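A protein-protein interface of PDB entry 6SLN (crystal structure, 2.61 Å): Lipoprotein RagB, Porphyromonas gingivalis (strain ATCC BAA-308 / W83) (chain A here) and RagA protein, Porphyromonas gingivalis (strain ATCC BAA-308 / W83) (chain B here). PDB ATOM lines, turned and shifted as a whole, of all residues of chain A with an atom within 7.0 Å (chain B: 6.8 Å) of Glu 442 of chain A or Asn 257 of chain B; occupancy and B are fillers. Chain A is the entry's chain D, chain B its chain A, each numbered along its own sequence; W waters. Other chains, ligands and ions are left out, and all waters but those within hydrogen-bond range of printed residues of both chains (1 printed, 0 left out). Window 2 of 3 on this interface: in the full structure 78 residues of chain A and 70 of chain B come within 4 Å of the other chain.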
ATOM      1  N   LYS A 328     -19.772  13.020 -11.822  1.00  0.00           N
ATOM      2  CA  LYS A 328     -19.002  12.432 -12.921  1.00  0.00           C
ATOM      3  C   LYS A 328     -17.631  13.110 -13.019  1.00  0.00           C
ATOM      4  O   LYS A 328     -17.205  13.589 -14.081  1.00  0.00           O
ATOM      5  CB  LYS A 328     -19.767  12.512 -14.243  1.00  0.00           C
ATOM      6  CG  LYS A 328     -20.922  11.526 -14.315  1.00  0.00           C
ATOM      7  CD  LYS A 328     -21.799  11.718 -15.551  1.00  0.00           C
ATOM      8  CE  LYS A 328     -21.357  10.873 -16.732  1.00  0.00           C
ATOM      9  NZ  LYS A 328     -21.970  11.434 -17.960  1.00  0.00           N
ATOM     10  N   THR A 437     -32.718  19.144 -16.926  1.00  0.00           N
ATOM     11  CA  THR A 437     -31.667  18.546 -16.126  1.00  0.00           C
ATOM     12  C   THR A 437     -30.301  18.969 -16.664  1.00  0.00           C
ATOM     13  O   THR A 437     -30.170  19.411 -17.805  1.00  0.00           O
ATOM     14  CB  THR A 437     -31.798  17.019 -16.113  1.00  0.00           C
ATOM     15  OG1 THR A 437     -31.806  16.508 -17.453  1.00  0.00           O
ATOM     16  CG2 THR A 437     -33.081  16.598 -15.390  1.00  0.00           C
ATOM     17  N   GLN A 438     -29.290  18.858 -15.813  1.00  0.00           N
ATOM     18  CA  GLN A 438     -27.916  19.200 -16.172  1.00  0.00           C
ATOM     19  C   GLN A 438     -27.472  18.430 -17.417  1.00  0.00           C
ATOM     20  O   GLN A 438     -27.438  17.191 -17.393  1.00  0.00           O
ATOM     21  CB  GLN A 438     -26.973  18.886 -15.006  1.00  0.00           C
ATOM     22  CG  GLN A 438     -27.378  19.476 -13.677  1.00  0.00           C
ATOM     23  CD  GLN A 438     -26.188  19.646 -12.747  1.00  0.00           C
ATOM     24  OE1 GLN A 438     -25.079  19.911 -13.195  1.00  0.00           O
ATOM     25  NE2 GLN A 438     -26.411  19.480 -11.450  1.00  0.00           N
ATOM     26  N   PRO A 439     -27.125  19.106 -18.515  1.00  0.00           N
ATOM     27  CA  PRO A 439     -26.799  18.343 -19.728  1.00  0.00           C
ATOM     28  C   PRO A 439     -25.545  17.495 -19.577  1.00  0.00           C
ATOM     29  O   PRO A 439     -25.531  16.337 -20.017  1.00  0.00           O
ATOM     30  CB  PRO A 439     -26.669  19.425 -20.814  1.00  0.00           C
ATOM     31  CG  PRO A 439     -26.640  20.720 -20.108  1.00  0.00           C
ATOM     32  CD  PRO A 439     -27.250  20.549 -18.767  1.00  0.00           C
ATOM     33  N   GLY A 440     -24.517  18.007 -18.908  1.00  0.00           N
ATOM     34  CA  GLY A 440     -23.298  17.251 -18.695  1.00  0.00           C
ATOM     35  C   GLY A 440     -23.514  15.915 -18.004  1.00  0.00           C
ATOM     36  O   GLY A 440     -22.624  15.054 -18.016  1.00  0.00           O
ATOM     37  N   LEU A 441     -24.698  15.723 -17.412  1.00  0.00           N
ATOM     38  CA  LEU A 441     -24.994  14.544 -16.609  1.00  0.00           C
ATOM     39  C   LEU A 441     -25.959  13.578 -17.282  1.00  0.00           C
ATOM     40  O   LEU A 441     -26.411  12.628 -16.627  1.00  0.00           O
ATOM     41  CB  LEU A 441     -25.553  14.950 -15.244  1.00  0.00           C
ATOM     42  CG  LEU A 441     -24.710  15.815 -14.314  1.00  0.00           C
ATOM     43  CD1 LEU A 441     -25.391  15.994 -12.962  1.00  0.00           C
ATOM     44  CD2 LEU A 441     -23.341  15.190 -14.136  1.00  0.00           C
ATOM     45  N   GLU A 442     -26.280  13.778 -18.566  1.00  0.00           N
ATOM     46  CA  GLU A 442     -27.279  12.919 -19.190  1.00  0.00           C
ATOM     47  C   GLU A 442     -26.782  11.485 -19.232  1.00  0.00           C
ATOM     48  O   GLU A 442     -25.595  11.226 -19.418  1.00  0.00           O
ATOM     49  CB  GLU A 442     -27.660  13.401 -20.594  1.00  0.00           C
ATOM     50  CG  GLU A 442     -28.985  14.269 -20.629  1.00  0.00           C
ATOM     51  CD  GLU A 442     -30.321  13.465 -20.483  1.00  0.00           C
ATOM     52  OE1 GLU A 442     -31.111  13.410 -21.459  1.00  0.00           O
ATOM     53  OE2 GLU A 442     -30.591  12.910 -19.388  1.00  0.00           O
ATOM     54  N   GLY A 443     -27.702  10.552 -19.015  1.00  0.00           N
ATOM     55  CA  GLY A 443     -27.390   9.174 -18.757  1.00  0.00           C
ATOM     56  C   GLY A 443     -27.340   8.842 -17.284  1.00  0.00           C
ATOM     57  O   GLY A 443     -27.643   7.707 -16.907  1.00  0.00           O
ATOM     58  N   PHE A 444     -26.969   9.814 -16.442  1.00  0.00           N
ATOM     59  CA  PHE A 444     -26.860   9.628 -14.997  1.00  0.00           C
ATOM     60  C   PHE A 444     -27.963  10.325 -14.202  1.00  0.00           C
ATOM     61  O   PHE A 444     -28.592   9.699 -13.340  1.00  0.00           O
ATOM     62  CB  PHE A 444     -25.478  10.106 -14.516  1.00  0.00           C
ATOM     63  CG  PHE A 444     -25.296  10.018 -13.039  1.00  0.00           C
ATOM     64  CD1 PHE A 444     -25.253   8.787 -12.413  1.00  0.00           C
ATOM     65  CD2 PHE A 444     -25.209  11.171 -12.268  1.00  0.00           C
ATOM     66  CE1 PHE A 444     -25.109   8.700 -11.034  1.00  0.00           C
ATOM     67  CE2 PHE A 444     -25.065  11.099 -10.898  1.00  0.00           C
ATOM     68  CZ  PHE A 444     -25.016   9.854 -10.274  1.00  0.00           C
ATOM     69  N   ALA A 445     -28.197  11.617 -14.451  1.00  0.00           N
ATOM     70  CA  ALA A 445     -29.281  12.390 -13.853  1.00  0.00           C
ATOM     71  C   ALA A 445     -30.315  12.662 -14.945  1.00  0.00           C
ATOM     72  O   ALA A 445     -30.155  13.588 -15.745  1.00  0.00           O
ATOM     73  CB  ALA A 445     -28.746  13.691 -13.267  1.00  0.00           C
ATOM     74  N   ASN A 446     -31.374  11.861 -14.989  1.00  0.00           N
ATOM     75  CA  ASN A 446     -32.293  12.010 -16.105  1.00  0.00           C
ATOM     76  C   ASN A 446     -33.626  12.583 -15.606  1.00  0.00           C
ATOM     77  O   ASN A 446     -33.666  13.276 -14.585  1.00  0.00           O
ATOM     78  CB  ASN A 446     -32.422  10.664 -16.823  1.00  0.00           C
ATOM     79  CG  ASN A 446     -31.069  10.060 -17.153  1.00  0.00           C
ATOM     80  OD1 ASN A 446     -30.187  10.743 -17.666  1.00  0.00           O
ATOM     81  ND2 ASN A 446     -30.890   8.780 -16.839  1.00  0.00           N
ATOM     82  N   THR A 447     -34.706  12.314 -16.332  1.00  0.00           N
ATOM     83  CA  THR A 447     -35.997  12.944 -16.069  1.00  0.00           C
ATOM     84  C   THR A 447     -36.934  11.894 -15.502  1.00  0.00           C
ATOM     85  O   THR A 447     -37.238  10.901 -16.166  1.00  0.00           O
ATOM     86  CB  THR A 447     -36.579  13.573 -17.334  1.00  0.00           C
ATOM     87  OG1 THR A 447     -35.665  14.548 -17.841  1.00  0.00           O
ATOM     88  CG2 THR A 447     -37.905  14.237 -17.054  1.00  0.00           C
ATOM     89  N   GLY B 253     -37.134   5.135 -20.357  1.00  0.00           N
ATOM     90  CA  GLY B 253     -36.570   6.460 -20.161  1.00  0.00           C
ATOM     91  C   GLY B 253     -35.574   6.560 -19.024  1.00  0.00           C
ATOM     92  O   GLY B 253     -35.063   7.659 -18.748  1.00  0.00           O
ATOM     93  N   PHE B 254     -35.275   5.436 -18.376  1.00  0.00           N
ATOM     94  CA  PHE B 254     -34.363   5.412 -17.244  1.00  0.00           C
ATOM     95  C   PHE B 254     -33.036   6.073 -17.559  1.00  0.00           C
ATOM     96  O   PHE B 254     -32.477   6.789 -16.721  1.00  0.00           O
ATOM     97  CB  PHE B 254     -34.123   3.975 -16.815  1.00  0.00           C
ATOM     98  CG  PHE B 254     -33.428   3.865 -15.522  1.00  0.00           C
ATOM     99  CD1 PHE B 254     -33.938   4.512 -14.401  1.00  0.00           C
ATOM    100  CD2 PHE B 254     -32.254   3.137 -15.410  1.00  0.00           C
ATOM    101  CE1 PHE B 254     -33.308   4.412 -13.192  1.00  0.00           C
ATOM    102  CE2 PHE B 254     -31.602   3.043 -14.180  1.00  0.00           C
ATOM    103  CZ  PHE B 254     -32.131   3.683 -13.067  1.00  0.00           C
ATOM    104  N   TRP B 255     -32.503   5.827 -18.747  1.00  0.00           N
ATOM    105  CA  TRP B 255     -31.185   6.301 -19.121  1.00  0.00           C
ATOM    106  C   TRP B 255     -31.228   7.634 -19.866  1.00  0.00           C
ATOM    107  O   TRP B 255     -30.203   8.078 -20.377  1.00  0.00           O
ATOM    108  CB  TRP B 255     -30.478   5.230 -19.958  1.00  0.00           C
ATOM    109  CG  TRP B 255     -30.308   3.901 -19.238  1.00  0.00           C
ATOM    110  CD1 TRP B 255     -30.927   2.718 -19.526  1.00  0.00           C
ATOM    111  CD2 TRP B 255     -29.458   3.638 -18.127  1.00  0.00           C
ATOM    112  NE1 TRP B 255     -30.523   1.736 -18.660  1.00  0.00           N
ATOM    113  CE2 TRP B 255     -29.616   2.275 -17.790  1.00  0.00           C
ATOM    114  CE3 TRP B 255     -28.584   4.423 -17.371  1.00  0.00           C
ATOM    115  CZ2 TRP B 255     -28.930   1.683 -16.730  1.00  0.00           C
ATOM    116  CZ3 TRP B 255     -27.908   3.837 -16.318  1.00  0.00           C
ATOM    117  CH2 TRP B 255     -28.086   2.480 -16.009  1.00  0.00           C
ATOM    118  N   GLY B 256     -32.372   8.293 -19.920  1.00  0.00           N
ATOM    119  CA  GLY B 256     -32.499   9.575 -20.579  1.00  0.00           C
ATOM    120  C   GLY B 256     -33.509   9.512 -21.704  1.00  0.00           C
ATOM    121  O   GLY B 256     -34.097   8.472 -21.997  1.00  0.00           O
ATOM    122  N   ASN B 257     -33.714  10.658 -22.328  1.00  0.00           N
ATOM    123  CA  ASN B 257     -34.561  10.708 -23.508  1.00  0.00           C
ATOM    124  C   ASN B 257     -33.695  10.586 -24.751  1.00  0.00           C
ATOM    125  O   ASN B 257     -32.502  10.896 -24.733  1.00  0.00           O
ATOM    126  CB  ASN B 257     -35.376  12.003 -23.539  1.00  0.00           C
ATOM    127  CG  ASN B 257     -35.854  12.418 -22.154  1.00  0.00           C
ATOM    128  OD1 ASN B 257     -35.702  13.572 -21.750  1.00  0.00           O
ATOM    129  ND2 ASN B 257     -36.435  11.473 -21.419  1.00  0.00           N
ATOM    130  N   ASN B 258     -34.302  10.108 -25.833  1.00  0.00           N
ATOM    131  CA  ASN B 258     -33.588   9.915 -27.092  1.00  0.00           C
ATOM    132  C   ASN B 258     -32.364   9.036 -26.868  1.00  0.00           C
ATOM    133  O   ASN B 258     -31.252   9.332 -27.308  1.00  0.00           O
ATOM    134  CB  ASN B 258     -33.197  11.254 -27.715  1.00  0.00           C
ATOM    135  CG  ASN B 258     -34.403  12.063 -28.161  1.00  0.00           C
ATOM    136  OD1 ASN B 258     -35.151  12.597 -27.336  1.00  0.00           O
ATOM    137  ND2 ASN B 258     -34.596  12.163 -29.476  1.00  0.00           N
ATOM    138  N   GLN B 259     -32.578   7.958 -26.134  1.00  0.00           N
ATOM    139  CA  GLN B 259     -31.532   7.000 -25.845  1.00  0.00           C
ATOM    140  C   GLN B 259     -31.685   5.788 -26.757  1.00  0.00           C
ATOM    141  O   GLN B 259     -32.789   5.455 -27.198  1.00  0.00           O
ATOM    142  CB  GLN B 259     -31.589   6.584 -24.374  1.00  0.00           C
ATOM    143  CG  GLN B 259     -30.300   6.030 -23.854  1.00  0.00           C
ATOM    144  CD  GLN B 259     -29.195   7.068 -23.767  1.00  0.00           C
ATOM    145  OE1 GLN B 259     -28.449   7.271 -24.727  1.00  0.00           O
ATOM    146  NE2 GLN B 259     -29.057   7.702 -22.602  1.00  0.00           N
ATOM    147  N   THR B 260     -30.562   5.152 -27.069  1.00  0.00           N
ATOM    148  CA  THR B 260     -30.549   3.872 -27.758  1.00  0.00           C
ATOM    149  C   THR B 260     -29.841   2.850 -26.881  1.00  0.00           C
ATOM    150  O   THR B 260     -29.230   3.186 -25.869  1.00  0.00           O
ATOM    151  CB  THR B 260     -29.855   3.966 -29.122  1.00  0.00           C
ATOM    152  OG1 THR B 260     -28.435   4.027 -28.925  1.00  0.00           O
ATOM    153  CG2 THR B 260     -30.329   5.188 -29.892  1.00  0.00           C
ATOM    154  N   MET B 267     -21.911   3.943 -22.566  1.00  0.00           N
ATOM    155  CA  MET B 267     -21.765   4.688 -21.320  1.00  0.00           C
ATOM    156  C   MET B 267     -21.421   3.766 -20.151  1.00  0.00           C
ATOM    157  O   MET B 267     -20.516   4.073 -19.356  1.00  0.00           O
ATOM    158  CB  MET B 267     -23.038   5.487 -21.050  1.00  0.00           C
ATOM    159  CG  MET B 267     -23.067   6.166 -19.691  1.00  0.00           C
ATOM    160  SD  MET B 267     -24.681   6.880 -19.313  1.00  0.00           S
ATOM    161  CE  MET B 267     -25.618   5.418 -18.873  1.00  0.00           C
ATOM    162  N   TYR B 417     -22.982   0.837 -12.721  1.00  0.00           N
ATOM    163  CA  TYR B 417     -22.795   2.157 -13.325  1.00  0.00           C
ATOM    164  C   TYR B 417     -22.983   3.262 -12.284  1.00  0.00           C
ATOM    165  O   TYR B 417     -23.863   3.185 -11.420  1.00  0.00           O
ATOM    166  CB  TYR B 417     -23.753   2.378 -14.504  1.00  0.00           C
ATOM    167  CG  TYR B 417     -23.599   3.772 -15.087  1.00  0.00           C
ATOM    168  CD1 TYR B 417     -22.500   4.097 -15.877  1.00  0.00           C
ATOM    169  CD2 TYR B 417     -24.523   4.775 -14.822  1.00  0.00           C
ATOM    170  CE1 TYR B 417     -22.329   5.379 -16.396  1.00  0.00           C
ATOM    171  CE2 TYR B 417     -24.359   6.069 -15.345  1.00  0.00           C
ATOM    172  CZ  TYR B 417     -23.250   6.358 -16.125  1.00  0.00           C
ATOM    173  OH  TYR B 417     -23.068   7.618 -16.646  1.00  0.00           O
HETATM  174  O   HOH W   1     -35.404  10.560 -19.153  1.00  0.00           O
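Of the printed residues of chain B, Lys 328 of chain A touches Tyr 417 (3.7 Å).
Of chain B, only Asn 257 (3.9 Å) comes within 4 Å of Glu 442 of chain A.
Of the printed residues of chain A, Phe 254 of chain B touches Asn 446.
Printed residues of chain A within 4 Å of Gly 256 of chain B: Asn 446.
Of the printed residues of chain A, Met 267 of chain B touches Gly 443 (3.6 Å).
Printed residues of chain A within 4 Å of Tyr 417 of chain B: Lys 328 (3.7 Å) and Gly 443 (3.99 Å).
The nearest residue of chain B that does not touch Glu 442 of chain A is Gly 256 of chain B (4.02 Å).
The nearest residue of chain A that does not touch Asn 257 of chain B is Thr 447 of chain A (4.03 Å).
The nearest printed residue of chain A that does not touch Trp 255 of chain B is Glu 442 of chain A (4.9 Å).
The backbone carbonyl oxygen (O) of Trp 255 of chain B lies within hydrogen-bond range of the side-chain amide nitrogen (NE2) of Gln 259 of chain B (2.5 Å).
The side-chain hydroxyl of Tyr 417 of chain B lies within hydrogen-bond range of the side-chain sulfur of Met 267 of chain B.
OD1 of Asn 446 of chain A sits close to OE2 of Glu 442 of chain A.
N of Gly 443 of chain A lies within hydrogen-bond range of OD1 of Asn 446 of chain A (2.8 Å).
Of the 10 printed residues of chain B, 6 touch a printed residue of chain A.
Printed residues of chain A that touch a printed residue of chain B: Lys 328, Glu 442, Gly 443 and Asn 446.
Among the printed residues, no Asp or Glu carboxylate lies within 4 Å of a Lys or Arg side-chain nitrogen of the other chain.
O of Phe 254 of chain B sits at hydrogen-bond distance from ND2 of Asn 446 of chain A (2.5 Å).
The side-chain amide nitrogen (ND2) of Asn 446 of chain A sits close to the backbone NH (N) of Gly 256 of chain B (3.5 Å).
Water W1 lies within hydrogen-bond range of ND2 of Asn 257 of chain B (2.7 Å), O of Gly 253 of chain B (2.9 Å) and N of Thr 447 of chain A (3.4 Å).
Tyr 417 of chain B touches Lys 328 of chain A.
N of Asn 257 of chain B touches OE1 of Glu 442 of chain A (3.9 Å).
Gly 443 of chain A touches Trp 255 of chain B (CA to O, 3.4 Å).
Met 267 of chain B touches Gly 443 of chain A (SD to CA, 3.6 Å).
Tyr 417 of chain B touches Gly 443 of chain A.
Trp 255 of chain B touches Asn 446 of chain A (C to ND2, 3.3 Å).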
